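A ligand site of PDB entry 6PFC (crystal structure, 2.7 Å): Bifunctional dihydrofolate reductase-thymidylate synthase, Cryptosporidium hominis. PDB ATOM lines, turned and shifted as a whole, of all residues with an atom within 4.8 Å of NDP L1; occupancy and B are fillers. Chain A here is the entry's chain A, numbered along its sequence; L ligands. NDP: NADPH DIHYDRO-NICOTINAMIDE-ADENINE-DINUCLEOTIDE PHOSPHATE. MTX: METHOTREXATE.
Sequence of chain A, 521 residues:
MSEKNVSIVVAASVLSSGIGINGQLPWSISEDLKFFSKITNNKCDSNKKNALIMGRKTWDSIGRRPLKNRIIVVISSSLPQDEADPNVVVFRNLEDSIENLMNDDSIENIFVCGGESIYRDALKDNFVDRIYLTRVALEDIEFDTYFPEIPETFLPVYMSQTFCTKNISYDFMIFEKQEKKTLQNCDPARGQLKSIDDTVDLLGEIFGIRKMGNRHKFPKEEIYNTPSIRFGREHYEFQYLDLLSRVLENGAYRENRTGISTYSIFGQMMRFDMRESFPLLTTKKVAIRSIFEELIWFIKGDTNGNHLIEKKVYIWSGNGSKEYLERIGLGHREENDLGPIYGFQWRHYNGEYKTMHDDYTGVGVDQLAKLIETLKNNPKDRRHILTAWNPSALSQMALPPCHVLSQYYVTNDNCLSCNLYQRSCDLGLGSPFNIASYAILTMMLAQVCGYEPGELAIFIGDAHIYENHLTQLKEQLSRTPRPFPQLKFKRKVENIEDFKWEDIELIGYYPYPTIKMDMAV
OG of Ser 76 lies within hydrogen-bond range of O2X of NDP L1 (2.5 Å). N of Ser 77 lies within hydrogen-bond range of O3X of NDP L1 (2.9 Å). An oxygen (O3X) of NDP L1 sits at hydrogen-bond distance from the side-chain hydroxyl of Ser 77, at 2.5 Å. An oxygen (O2A) of NDP L1 lies within hydrogen-bond range of the backbone NH (N) of Thr 58, 3.2 Å away. The side-chain hydroxyl of Thr 58 sits at hydrogen-bond distance from an oxygen (O2A) of NDP L1 (2.6 Å). O1A of NDP L1 lies within hydrogen-bond range of OG of Ser 117 (2.6 Å). The backbone NH of Ala 11 sits at hydrogen-bond distance from an oxygen (O7N) of NDP L1, 3.0 Å away. The backbone carbonyl oxygen (O) of Ala 11 lies within hydrogen-bond range of a nitrogen (N7N) of NDP L1, at 2.7 Å. N of Glu 116 sits at hydrogen-bond distance from O2N of NDP L1. An oxygen (O2A) of NDP L1 lies within hydrogen-bond range of the backbone NH (N) of Gly 115 (3.0 Å). The backbone NH (N) of Gln 24 lies within hydrogen-bond range of an oxygen (O3D) of NDP L1 (3.1 Å). The backbone carbonyl oxygen (O) of Gln 24 is in hydrogen-bond range of an oxygen (O3D) of NDP L1, at 3.0 Å. N of Arg 56 lies within hydrogen-bond range of O4B of NDP L1 (3.2 Å). NH1 of Arg 56 is in salt-bridge range of O1X of NDP L1, 3.1 Å away. A nitrogen (N7N) of NDP L1 is in hydrogen-bond range of the backbone carbonyl oxygen (O) of Ile 19 (3.2 Å). O2X of NDP L1 is in hydrogen-bond range of OG of Ser 78, at 3.3 Å. N of Lys 57 sits at hydrogen-bond distance from O5B of NDP L1, 3.3 Å away. The backbone NH of Val 10 lies within hydrogen-bond range of a nitrogen (N3) of MTX L2 (3.3 Å). A nitrogen (NA2) of MTX L2 lies within hydrogen-bond range of the backbone carbonyl oxygen (O) of Val 10 (3.4 Å). The backbone carbonyl oxygen (O) of Val 9 is in hydrogen-bond range of a nitrogen (NA4) of MTX L2, at 2.6 Å.
O4B of NDP L1 sits close to O of Ile 75, at 3.3 Å. Val 10 touches NDP L1. CA of Gly 20 touches O3D of NDP L1 (3.5 Å). Ile 21 touches NDP L1 (N to O3D, 3.8 Å). Gly 23 touches NDP L1. Leu 25 touches NDP L1 (CD2 to C2N, 3.7 Å). Gly 55 touches NDP L1. O of Arg 92 touches C2A of NDP L1 (3.1 Å). Cys 113 touches NDP L1. Gly 114 touches NDP L1 (O to C5N, 3.9 Å). Ile 118 touches NDP L1 (CD1 to C8A, 3.95 Å). Tyr 119 touches NDP L1 (OH to C4N, 3.995 Å). Asp 121 touches NDP L1. OG1 of Thr 145 touches O1N of NDP L1, 3.6 Å away. Hydrophobic or aromatic side chains within 4 Å of NDP L1: Val 10, Ala 11, Ile 19, Leu 25, Ile 75 and Ile 118. Within 4 Å of NDP L1: Val 10, Ala 11, Ile 19, Gly 20, Ile 21, Gly 23, Gln 24, Leu 25, Gly 55, Arg 56, Lys 57, Thr 58, Ile 75, Ser 76, Ser 77, Ser 78, Arg 92, Cys 113, Gly 114, Gly 115, Glu 116, Ser 117, Ile 118, Tyr 119, Asp 121 and Thr 145.
The backbone NH of Ser 78 sits at hydrogen-bond distance from the side-chain hydroxyl of Ser 76 (3.2 Å). O of Ser 77 lies within hydrogen-bond range of NH1 of Arg 92. The side-chain hydroxyl (OG1) of Thr 58 lies within hydrogen-bond range of the backbone NH (N) of Gly 115, 3.3 Å away. The backbone carbonyl oxygen (O) of Thr 58 lies within hydrogen-bond range of the side-chain hydroxyl (OG) of Ser 61, at 2.7 Å. O of Ile 75 lies within hydrogen-bond range of N of Arg 56 (3.3 Å). The backbone carbonyl oxygen (O) of Cys 113 sits at hydrogen-bond distance from the side-chain hydroxyl (OH) of Tyr 119 (3.3 Å). The backbone NH of Gly 20 is in hydrogen-bond range of the backbone carbonyl oxygen of Thr 145 (3.4 Å). O of Gly 114 lies close to OH of Tyr 119 (3.5 Å).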
ATOM      1  N   VAL A   9      -1.960 -20.088  -2.474  1.00  0.00           N
ATOM      2  CA  VAL A   9      -2.344 -21.488  -2.341  1.00  0.00           C
ATOM      3  C   VAL A   9      -2.685 -21.742  -0.881  1.00  0.00           C
ATOM      4  O   VAL A   9      -1.870 -21.438   0.002  1.00  0.00           O
ATOM      5  CB  VAL A   9      -1.243 -22.436  -2.825  1.00  0.00           C
ATOM      6  CG1 VAL A   9      -1.791 -23.857  -2.982  1.00  0.00           C
ATOM      7  CG2 VAL A   9      -0.641 -21.946  -4.128  1.00  0.00           C
ATOM      8  N   VAL A  10      -3.884 -22.262  -0.615  1.00  0.00           N
ATOM      9  CA  VAL A  10      -4.360 -22.435   0.749  1.00  0.00           C
ATOM     10  C   VAL A  10      -5.394 -23.548   0.768  1.00  0.00           C
ATOM     11  O   VAL A  10      -6.102 -23.768  -0.216  1.00  0.00           O
ATOM     12  CB  VAL A  10      -4.933 -21.095   1.298  1.00  0.00           C
ATOM     13  CG1 VAL A  10      -6.107 -20.623   0.448  1.00  0.00           C
ATOM     14  CG2 VAL A  10      -5.338 -21.242   2.759  1.00  0.00           C
ATOM     15  N   ALA A  11      -5.464 -24.249   1.896  1.00  0.00           N
ATOM     16  CA  ALA A  11      -6.506 -25.234   2.178  1.00  0.00           C
ATOM     17  C   ALA A  11      -7.192 -24.817   3.468  1.00  0.00           C
ATOM     18  O   ALA A  11      -6.591 -24.853   4.545  1.00  0.00           O
ATOM     19  CB  ALA A  11      -5.918 -26.643   2.289  1.00  0.00           C
ATOM     20  N   ILE A  19      -7.270 -23.197   9.004  1.00  0.00           N
ATOM     21  CA  ILE A  19      -6.178 -23.743   8.189  1.00  0.00           C
ATOM     22  C   ILE A  19      -5.119 -24.426   9.055  1.00  0.00           C
ATOM     23  O   ILE A  19      -4.242 -25.117   8.539  1.00  0.00           O
ATOM     24  CB  ILE A  19      -5.516 -22.652   7.322  1.00  0.00           C
ATOM     25  CG1 ILE A  19      -4.827 -21.612   8.195  1.00  0.00           C
ATOM     26  CG2 ILE A  19      -6.554 -21.986   6.419  1.00  0.00           C
ATOM     27  CD1 ILE A  19      -3.996 -20.624   7.413  1.00  0.00           C
ATOM     28  N   GLY A  20      -5.182 -24.232  10.375  1.00  0.00           N
ATOM     29  CA  GLY A  20      -4.153 -24.787  11.230  1.00  0.00           C
ATOM     30  C   GLY A  20      -4.593 -24.905  12.669  1.00  0.00           C
ATOM     31  O   GLY A  20      -5.559 -24.271  13.113  1.00  0.00           O
ATOM     32  N   ILE A  21      -3.861 -25.733  13.421  1.00  0.00           N
ATOM     33  CA  ILE A  21      -4.079 -25.931  14.846  1.00  0.00           C
ATOM     34  C   ILE A  21      -2.808 -26.448  15.489  1.00  0.00           C
ATOM     35  O   ILE A  21      -2.229 -27.441  15.045  1.00  0.00           O
ATOM     36  CB  ILE A  21      -5.267 -26.892  15.102  1.00  0.00           C
ATOM     37  CG1 ILE A  21      -5.373 -27.214  16.591  1.00  0.00           C
ATOM     38  CG2 ILE A  21      -5.128 -28.165  14.292  1.00  0.00           C
ATOM     39  CD1 ILE A  21      -5.707 -26.018  17.466  1.00  0.00           C
ATOM     40  N   GLY A  23       0.238 -25.427  15.468  1.00  0.00           N
ATOM     41  CA  GLY A  23       1.401 -25.456  14.607  1.00  0.00           C
ATOM     42  C   GLY A  23       1.398 -26.526  13.529  1.00  0.00           C
ATOM     43  O   GLY A  23       2.441 -26.762  12.916  1.00  0.00           O
ATOM     44  N   GLN A  24       0.266 -27.164  13.278  1.00  0.00           N
ATOM     45  CA  GLN A  24       0.174 -28.177  12.245  1.00  0.00           C
ATOM     46  C   GLN A  24      -1.213 -28.115  11.605  1.00  0.00           C
ATOM     47  O   GLN A  24      -2.064 -27.307  12.001  1.00  0.00           O
ATOM     48  CB  GLN A  24       0.459 -29.580  12.801  1.00  0.00           C
ATOM     49  CG  GLN A  24      -0.541 -30.055  13.835  1.00  0.00           C
ATOM     50  CD  GLN A  24      -0.216 -31.456  14.328  1.00  0.00           C
ATOM     51  OE1 GLN A  24       0.900 -31.941  14.166  1.00  0.00           O
ATOM     52  NE2 GLN A  24      -1.203 -32.116  14.946  1.00  0.00           N
ATOM     53  N   LEU A  25      -1.432 -28.965  10.606  1.00  0.00           N
ATOM     54  CA  LEU A  25      -2.704 -28.982   9.879  1.00  0.00           C
ATOM     55  C   LEU A  25      -3.759 -29.744  10.676  1.00  0.00           C
ATOM     56  O   LEU A  25      -3.435 -30.709  11.377  1.00  0.00           O
ATOM     57  CB  LEU A  25      -2.526 -29.630   8.506  1.00  0.00           C
ATOM     58  CG  LEU A  25      -1.548 -28.944   7.546  1.00  0.00           C
ATOM     59  CD1 LEU A  25      -1.346 -29.785   6.297  1.00  0.00           C
ATOM     60  CD2 LEU A  25      -2.046 -27.555   7.181  1.00  0.00           C
ATOM     61  N   TRP A  27      -5.918 -31.692   9.481  1.00  0.00           N
ATOM     62  CA  TRP A  27      -6.341 -32.834   8.682  1.00  0.00           C
ATOM     63  C   TRP A  27      -5.115 -33.405   7.966  1.00  0.00           C
ATOM     64  O   TRP A  27      -4.055 -32.780   7.919  1.00  0.00           O
ATOM     65  CB  TRP A  27      -7.422 -32.438   7.665  1.00  0.00           C
ATOM     66  CG  TRP A  27      -7.038 -31.247   6.844  1.00  0.00           C
ATOM     67  CD1 TRP A  27      -6.066 -31.182   5.884  1.00  0.00           C
ATOM     68  CD2 TRP A  27      -7.628 -29.936   6.904  1.00  0.00           C
ATOM     69  NE1 TRP A  27      -6.006 -29.914   5.354  1.00  0.00           N
ATOM     70  CE2 TRP A  27      -6.962 -29.139   5.952  1.00  0.00           C
ATOM     71  CE3 TRP A  27      -8.661 -29.375   7.659  1.00  0.00           C
ATOM     72  CZ2 TRP A  27      -7.285 -27.798   5.752  1.00  0.00           C
ATOM     73  CZ3 TRP A  27      -8.979 -28.041   7.455  1.00  0.00           C
ATOM     74  CH2 TRP A  27      -8.295 -27.275   6.509  1.00  0.00           C
ATOM     75  N   GLY A  55       5.516 -17.868   5.827  1.00  0.00           N
ATOM     76  CA  GLY A  55       5.932 -17.344   7.107  1.00  0.00           C
ATOM     77  C   GLY A  55       6.886 -18.270   7.828  1.00  0.00           C
ATOM     78  O   GLY A  55       7.118 -19.409   7.426  1.00  0.00           O
ATOM     79  N   ARG A  56       7.437 -17.765   8.934  1.00  0.00           N
ATOM     80  CA  ARG A  56       8.436 -18.532   9.672  1.00  0.00           C
ATOM     81  C   ARG A  56       7.817 -19.751  10.363  1.00  0.00           C
ATOM     82  O   ARG A  56       8.410 -20.835  10.367  1.00  0.00           O
ATOM     83  CB  ARG A  56       9.142 -17.656  10.702  1.00  0.00           C
ATOM     84  CG  ARG A  56      10.357 -18.304  11.341  1.00  0.00           C
ATOM     85  CD  ARG A  56      10.475 -17.968  12.811  1.00  0.00           C
ATOM     86  NE  ARG A  56       9.545 -18.733  13.639  1.00  0.00           N
ATOM     87  CZ  ARG A  56       9.077 -18.317  14.811  1.00  0.00           C
ATOM     88  NH1 ARG A  56       9.456 -17.146  15.309  1.00  0.00           N
ATOM     89  NH2 ARG A  56       8.238 -19.076  15.504  1.00  0.00           N
ATOM     90  N   LYS A  57       6.634 -19.579  10.960  1.00  0.00           N
ATOM     91  CA  LYS A  57       5.997 -20.700  11.636  1.00  0.00           C
ATOM     92  C   LYS A  57       5.599 -21.795  10.665  1.00  0.00           C
ATOM     93  O   LYS A  57       5.659 -22.984  11.008  1.00  0.00           O
ATOM     94  CB  LYS A  57       4.790 -20.213  12.436  1.00  0.00           C
ATOM     95  CG  LYS A  57       5.143 -19.228  13.539  1.00  0.00           C
ATOM     96  CD  LYS A  57       3.983 -18.993  14.493  1.00  0.00           C
ATOM     97  CE  LYS A  57       4.370 -18.026  15.599  1.00  0.00           C
ATOM     98  NZ  LYS A  57       3.271 -17.831  16.582  1.00  0.00           N
ATOM     99  N   THR A  58       5.199 -21.435   9.445  1.00  0.00           N
ATOM    100  CA  THR A  58       4.980 -22.437   8.408  1.00  0.00           C
ATOM    101  C   THR A  58       6.286 -23.109   8.017  1.00  0.00           C
ATOM    102  O   THR A  58       6.331 -24.313   7.760  1.00  0.00           O
ATOM    103  CB  THR A  58       4.297 -21.796   7.200  1.00  0.00           C
ATOM    104  OG1 THR A  58       3.062 -21.205   7.606  1.00  0.00           O
ATOM    105  CG2 THR A  58       4.020 -22.850   6.122  1.00  0.00           C
ATOM    106  N   SER A  61       6.809 -25.744  10.482  1.00  0.00           N
ATOM    107  CA  SER A  61       5.891 -26.872  10.383  1.00  0.00           C
ATOM    108  C   SER A  61       6.279 -27.846   9.285  1.00  0.00           C
ATOM    109  O   SER A  61       5.847 -29.006   9.328  1.00  0.00           O
ATOM    110  CB  SER A  61       4.461 -26.368  10.156  1.00  0.00           C
ATOM    111  OG  SER A  61       4.370 -25.658   8.938  1.00  0.00           O
ATOM    112  N   ILE A  75       9.611 -15.435   5.487  1.00  0.00           N
ATOM    113  CA  ILE A  75       9.450 -14.118   6.091  1.00  0.00           C
ATOM    114  C   ILE A  75       9.709 -14.256   7.594  1.00  0.00           C
ATOM    115  O   ILE A  75       8.981 -14.967   8.290  1.00  0.00           O
ATOM    116  CB  ILE A  75       8.043 -13.546   5.835  1.00  0.00           C
ATOM    117  CG1 ILE A  75       7.763 -13.486   4.334  1.00  0.00           C
ATOM    118  CG2 ILE A  75       7.911 -12.169   6.451  1.00  0.00           C
ATOM    119  CD1 ILE A  75       8.808 -12.721   3.565  1.00  0.00           C
ATOM    120  N   SER A  76      10.735 -13.570   8.079  1.00  0.00           N
ATOM    121  CA  SER A  76      11.069 -13.631   9.496  1.00  0.00           C
ATOM    122  C   SER A  76      11.903 -12.413   9.863  1.00  0.00           C
ATOM    123  O   SER A  76      12.648 -11.880   9.036  1.00  0.00           O
ATOM    124  CB  SER A  76      11.829 -14.914   9.838  1.00  0.00           C
ATOM    125  OG  SER A  76      12.160 -14.953  11.217  1.00  0.00           O
ATOM    126  N   SER A  77      11.764 -11.990  11.116  1.00  0.00           N
ATOM    127  CA  SER A  77      12.558 -10.891  11.655  1.00  0.00           C
ATOM    128  C   SER A  77      13.787 -11.368  12.408  1.00  0.00           C
ATOM    129  O   SER A  77      14.662 -10.547  12.716  1.00  0.00           O
ATOM    130  CB  SER A  77      11.690 -10.024  12.586  1.00  0.00           C
ATOM    131  OG  SER A  77      11.208 -10.784  13.674  1.00  0.00           O
ATOM    132  N   SER A  78      13.882 -12.656  12.722  1.00  0.00           N
ATOM    133  CA  SER A  78      14.988 -13.189  13.510  1.00  0.00           C
ATOM    134  C   SER A  78      15.853 -14.194  12.763  1.00  0.00           C
ATOM    135  O   SER A  78      17.026 -14.355  13.119  1.00  0.00           O
ATOM    136  CB  SER A  78      14.458 -13.840  14.795  1.00  0.00           C
ATOM    137  OG  SER A  78      13.561 -14.907  14.496  1.00  0.00           O
ATOM    138  N   ARG A  92      13.037  -9.723   5.598  1.00  0.00           N
ATOM    139  CA  ARG A  92      12.569  -9.144   6.857  1.00  0.00           C
ATOM    140  C   ARG A  92      11.098  -8.741   6.819  1.00  0.00           C
ATOM    141  O   ARG A  92      10.478  -8.630   7.878  1.00  0.00           O
ATOM    142  CB  ARG A  92      13.420  -7.928   7.226  1.00  0.00           C
ATOM    143  CG  ARG A  92      14.882  -8.247   7.459  1.00  0.00           C
ATOM    144  CD  ARG A  92      15.048  -9.350   8.478  1.00  0.00           C
ATOM    145  NE  ARG A  92      16.433  -9.796   8.581  1.00  0.00           N
ATOM    146  CZ  ARG A  92      16.829 -10.860   9.280  1.00  0.00           C
ATOM    147  NH1 ARG A  92      15.945 -11.582   9.946  1.00  0.00           N
ATOM    148  NH2 ARG A  92      18.110 -11.194   9.302  1.00  0.00           N
ATOM    149  N   ASN A  93      10.529  -8.519   5.636  1.00  0.00           N
ATOM    150  CA  ASN A  93       9.115  -8.191   5.518  1.00  0.00           C
ATOM    151  C   ASN A  93       8.586  -8.702   4.183  1.00  0.00           C
ATOM    152  O   ASN A  93       9.352  -9.036   3.272  1.00  0.00           O
ATOM    153  CB  ASN A  93       8.880  -6.676   5.636  1.00  0.00           C
ATOM    154  CG  ASN A  93       9.588  -5.879   4.561  1.00  0.00           C
ATOM    155  OD1 ASN A  93       9.057  -5.658   3.473  1.00  0.00           O
ATOM    156  ND2 ASN A  93      10.812  -5.447   4.865  1.00  0.00           N
ATOM    157  N   CYS A 113       2.234 -19.086   0.311  1.00  0.00           N
ATOM    158  CA  CYS A 113       1.824 -20.277   1.031  1.00  0.00           C
ATOM    159  C   CYS A 113       1.806 -20.111   2.538  1.00  0.00           C
ATOM    160  O   CYS A 113       1.342 -21.025   3.238  1.00  0.00           O
ATOM    161  CB  CYS A 113       2.756 -21.454   0.677  1.00  0.00           C
ATOM    162  SG  CYS A 113       3.335 -21.466  -1.033  1.00  0.00           S
ATOM    163  N   GLY A 114       2.281 -18.983   3.070  1.00  0.00           N
ATOM    164  CA  GLY A 114       2.465 -18.795   4.495  1.00  0.00           C
ATOM    165  C   GLY A 114       1.195 -18.823   5.325  1.00  0.00           C
ATOM    166  O   GLY A 114       0.099 -19.052   4.792  1.00  0.00           O
ATOM    167  N   GLY A 115       1.326 -18.599   6.626  1.00  0.00           N
ATOM    168  CA  GLY A 115       0.193 -18.660   7.529  1.00  0.00           C
ATOM    169  C   GLY A 115      -0.764 -17.496   7.425  1.00  0.00           C
ATOM    170  O   GLY A 115      -0.793 -16.783   6.417  1.00  0.00           O
ATOM    171  N   GLU A 116      -1.560 -17.283   8.481  1.00  0.00           N
ATOM    172  CA  GLU A 116      -2.562 -16.223   8.476  1.00  0.00           C
ATOM    173  C   GLU A 116      -1.928 -14.851   8.306  1.00  0.00           C
ATOM    174  O   GLU A 116      -2.457 -14.003   7.586  1.00  0.00           O
ATOM    175  CB  GLU A 116      -3.391 -16.293   9.764  1.00  0.00           C
ATOM    176  CG  GLU A 116      -4.416 -15.188   9.907  1.00  0.00           C
ATOM    177  CD  GLU A 116      -5.356 -15.420  11.073  1.00  0.00           C
ATOM    178  OE1 GLU A 116      -5.291 -16.506  11.689  1.00  0.00           O
ATOM    179  OE2 GLU A 116      -6.161 -14.521  11.389  1.00  0.00           O
ATOM    180  N   SER A 117      -0.793 -14.615   8.971  1.00  0.00           N
ATOM    181  CA  SER A 117      -0.158 -13.306   8.898  1.00  0.00           C
ATOM    182  C   SER A 117       0.302 -12.990   7.474  1.00  0.00           C
ATOM    183  O   SER A 117       0.184 -11.840   7.026  1.00  0.00           O
ATOM    184  CB  SER A 117       1.024 -13.244   9.863  1.00  0.00           C
ATOM    185  OG  SER A 117       2.037 -14.174   9.506  1.00  0.00           O
ATOM    186  N   ILE A 118       0.829 -13.981   6.760  1.00  0.00           N
ATOM    187  CA  ILE A 118       1.294 -13.743   5.394  1.00  0.00           C
ATOM    188  C   ILE A 118       0.111 -13.584   4.450  1.00  0.00           C
ATOM    189  O   ILE A 118       0.146 -12.738   3.545  1.00  0.00           O
ATOM    190  CB  ILE A 118       2.238 -14.881   4.953  1.00  0.00           C
ATOM    191  CG1 ILE A 118       3.385 -15.033   5.950  1.00  0.00           C
ATOM    192  CG2 ILE A 118       2.794 -14.609   3.562  1.00  0.00           C
ATOM    193  CD1 ILE A 118       4.216 -13.789   6.119  1.00  0.00           C
ATOM    194  N   TYR A 119      -0.930 -14.396   4.625  1.00  0.00           N
ATOM    195  CA  TYR A 119      -2.123 -14.274   3.791  1.00  0.00           C
ATOM    196  C   TYR A 119      -2.776 -12.902   3.965  1.00  0.00           C
ATOM    197  O   TYR A 119      -3.145 -12.246   2.983  1.00  0.00           O
ATOM    198  CB  TYR A 119      -3.121 -15.374   4.125  1.00  0.00           C
ATOM    199  CG  TYR A 119      -2.738 -16.748   3.605  1.00  0.00           C
ATOM    200  CD1 TYR A 119      -2.038 -16.897   2.417  1.00  0.00           C
ATOM    201  CD2 TYR A 119      -3.104 -17.888   4.304  1.00  0.00           C
ATOM    202  CE1 TYR A 119      -1.696 -18.147   1.947  1.00  0.00           C
ATOM    203  CE2 TYR A 119      -2.764 -19.147   3.844  1.00  0.00           C
ATOM    204  CZ  TYR A 119      -2.069 -19.276   2.664  1.00  0.00           C
ATOM    205  OH  TYR A 119      -1.735 -20.528   2.208  1.00  0.00           O
ATOM    206  N   ASP A 121      -1.514 -10.003   5.077  1.00  0.00           N
ATOM    207  CA  ASP A 121      -0.696  -8.905   4.580  1.00  0.00           C
ATOM    208  C   ASP A 121      -0.532  -8.931   3.069  1.00  0.00           C
ATOM    209  O   ASP A 121      -0.230  -7.888   2.480  1.00  0.00           O
ATOM    210  CB  ASP A 121       0.679  -8.917   5.260  1.00  0.00           C
ATOM    211  CG  ASP A 121       0.608  -8.536   6.732  1.00  0.00           C
ATOM    212  OD1 ASP A 121      -0.308  -7.769   7.104  1.00  0.00           O
ATOM    213  OD2 ASP A 121       1.481  -8.987   7.495  1.00  0.00           O
ATOM    214  N   THR A 145      -5.779 -20.859  13.650  1.00  0.00           N
ATOM    215  CA  THR A 145      -5.256 -20.089  12.533  1.00  0.00           C
ATOM    216  C   THR A 145      -6.255 -20.175  11.394  1.00  0.00           C
ATOM    217  O   THR A 145      -6.666 -21.272  11.010  1.00  0.00           O
ATOM    218  CB  THR A 145      -3.872 -20.606  12.096  1.00  0.00           C
ATOM    219  OG1 THR A 145      -2.980 -20.565  13.208  1.00  0.00           O
ATOM    220  CG2 THR A 145      -3.321 -19.751  10.975  1.00  0.00           C
HETATM  221  PA  NDP L   1       2.930 -17.853   9.976  1.00  0.00           P
HETATM  222  O1A NDP L   1       2.076 -16.782   9.321  1.00  0.00           O
HETATM  223  O2A NDP L   1       3.079 -19.012   9.029  1.00  0.00           O
HETATM  224  O5B NDP L   1       4.325 -17.294  10.262  1.00  0.00           O
HETATM  225  C5B NDP L   1       4.494 -16.207  11.150  1.00  0.00           C
HETATM  226  C4B NDP L   1       5.852 -15.664  11.279  1.00  0.00           C
HETATM  227  O4B NDP L   1       6.237 -15.019  10.085  1.00  0.00           O
HETATM  228  C3B NDP L   1       5.944 -14.637  12.314  1.00  0.00           C
HETATM  229  O3B NDP L   1       6.154 -15.184  13.572  1.00  0.00           O
HETATM  230  C2B NDP L   1       7.096 -13.883  11.878  1.00  0.00           C
HETATM  231  O2B NDP L   1       8.287 -14.565  12.156  1.00  0.00           O
HETATM  232  C1B NDP L   1       6.923 -13.830  10.437  1.00  0.00           C
HETATM  233  N9A NDP L   1       6.181 -12.668  10.080  1.00  0.00           N
HETATM  234  C8A NDP L   1       4.837 -12.611   9.839  1.00  0.00           C
HETATM  235  N7A NDP L   1       4.506 -11.347   9.522  1.00  0.00           N
HETATM  236  C5A NDP L   1       5.640 -10.578   9.553  1.00  0.00           C
HETATM  237  C6A NDP L   1       5.920  -9.199   9.318  1.00  0.00           C
HETATM  238  N6A NDP L   1       4.811  -8.294   8.941  1.00  0.00           N
HETATM  239  N1A NDP L   1       7.190  -8.732   9.426  1.00  0.00           N
HETATM  240  C2A NDP L   1       8.187  -9.592   9.767  1.00  0.00           C
HETATM  241  N3A NDP L   1       7.973 -10.891  10.011  1.00  0.00           N
HETATM  242  C4A NDP L   1       6.702 -11.416   9.901  1.00  0.00           C
HETATM  243  O3  NDP L   1       2.271 -18.344  11.341  1.00  0.00           O
HETATM  244  PN  NDP L   1       0.792 -18.922  11.399  1.00  0.00           P
HETATM  245  O1N NDP L   1       0.392 -19.248  12.848  1.00  0.00           O
HETATM  246  O2N NDP L   1      -0.157 -17.872  10.854  1.00  0.00           O
HETATM  247  O5D NDP L   1       0.712 -20.269  10.507  1.00  0.00           O
HETATM  248  C5D NDP L   1       0.870 -21.534  11.114  1.00  0.00           C
HETATM  249  C4D NDP L   1      -0.233 -22.480  11.013  1.00  0.00           C
HETATM  250  O4D NDP L   1      -0.892 -22.330   9.754  1.00  0.00           O
HETATM  251  C3D NDP L   1       0.255 -23.863  11.066  1.00  0.00           C
HETATM  252  O3D NDP L   1      -0.672 -24.654  11.737  1.00  0.00           O
HETATM  253  C2D NDP L   1       0.315 -24.249   9.701  1.00  0.00           C
HETATM  254  O2D NDP L   1       0.218 -25.636   9.582  1.00  0.00           O
HETATM  255  C1D NDP L   1      -0.860 -23.567   9.131  1.00  0.00           C
HETATM  256  N1N NDP L   1      -0.756 -23.444   7.697  1.00  0.00           N
HETATM  257  C2N NDP L   1      -1.778 -23.882   6.951  1.00  0.00           C
HETATM  258  C3N NDP L   1      -1.729 -23.797   5.547  1.00  0.00           C
HETATM  259  C7N NDP L   1      -2.914 -24.303   4.738  1.00  0.00           C
HETATM  260  O7N NDP L   1      -2.918 -24.139   3.504  1.00  0.00           O
HETATM  261  N7N NDP L   1      -4.025 -24.949   5.375  1.00  0.00           N
HETATM  262  C4N NDP L   1      -0.599 -23.240   4.913  1.00  0.00           C
HETATM  263  C5N NDP L   1       0.443 -22.789   5.732  1.00  0.00           C
HETATM  264  C6N NDP L   1       0.359 -22.903   7.113  1.00  0.00           C
HETATM  265  P2B NDP L   1       9.304 -14.021  13.203  1.00  0.00           P
HETATM  266  O1X NDP L   1       8.699 -14.198  14.607  1.00  0.00           O
HETATM  267  O2X NDP L   1      10.558 -14.788  13.088  1.00  0.00           O
HETATM  268  O3X NDP L   1       9.623 -12.585  12.952  1.00  0.00           O
HETATM  269  N1  MTX L   2      -2.669 -27.163   1.144  1.00  0.00           N
HETATM  270  C2  MTX L   2      -3.017 -26.258   0.213  1.00  0.00           C
HETATM  271  NA2 MTX L   2      -4.153 -26.536  -0.633  1.00  0.00           N
HETATM  272  N3  MTX L   2      -2.339 -25.114   0.045  1.00  0.00           N
HETATM  273  C4  MTX L   2      -1.274 -24.824   0.825  1.00  0.00           C
HETATM  274  NA4 MTX L   2      -0.526 -23.617   0.674  1.00  0.00           N
HETATM  275  C4A MTX L   2      -0.873 -25.752   1.816  1.00  0.00           C
HETATM  276  N5  MTX L   2       0.200 -25.506   2.628  1.00  0.00           N
HETATM  277  C6  MTX L   2       0.538 -26.416   3.552  1.00  0.00           C
HETATM  278  C7  MTX L   2      -0.181 -27.606   3.717  1.00  0.00           C
HETATM  279  N8  MTX L   2      -1.236 -27.841   2.911  1.00  0.00           N
HETATM  280  C8A MTX L   2      -1.603 -26.923   1.957  1.00  0.00           C
HETATM  281  C9  MTX L   2       1.730 -26.138   4.449  1.00  0.00           C
HETATM  282  N10 MTX L   2       2.447 -27.313   4.885  1.00  0.00           N
HETATM  283  CM  MTX L   2       2.507 -27.632   6.293  1.00  0.00           C
HETATM  284  C11 MTX L   2       4.374 -29.852   2.062  1.00  0.00           C
HETATM  285  C12 MTX L   2       3.848 -30.359   3.244  1.00  0.00           C
HETATM  286  C13 MTX L   2       3.225 -29.524   4.161  1.00  0.00           C
HETATM  287  C14 MTX L   2       3.118 -28.168   3.905  1.00  0.00           C
HETATM  288  C15 MTX L   2       3.629 -27.644   2.723  1.00  0.00           C
HETATM  289  C16 MTX L   2       4.257 -28.486   1.801  1.00  0.00           C
HETATM  290  C   MTX L   2       5.044 -30.778   1.077  1.00  0.00           C
HETATM  291  O   MTX L   2       5.637 -31.760   1.505  1.00  0.00           O
HETATM  292  N   MTX L   2       5.006 -30.557  -0.355  1.00  0.00           N
HETATM  293  CA  MTX L   2       5.657 -31.471  -1.248  1.00  0.00           C
HETATM  294  CT  MTX L   2       6.084 -30.727  -2.449  1.00  0.00           C
HETATM  295  O1  MTX L   2       5.827 -29.499  -2.550  1.00  0.00           O
HETATM  296  O2  MTX L   2       6.718 -31.321  -3.382  1.00  0.00           O
HETATM  297  CB  MTX L   2       4.670 -32.487  -1.696  1.00  0.00           C
HETATM  298  CG  MTX L   2       4.488 -33.741  -0.898  1.00  0.00           C
HETATM  299  CD  MTX L   2       3.733 -34.839  -1.570  1.00  0.00           C
HETATM  300  OE1 MTX L   2       3.860 -34.975  -2.804  1.00  0.00           O
HETATM  301  OE2 MTX L   2       2.703 -35.300  -1.019  1.00  0.00           O
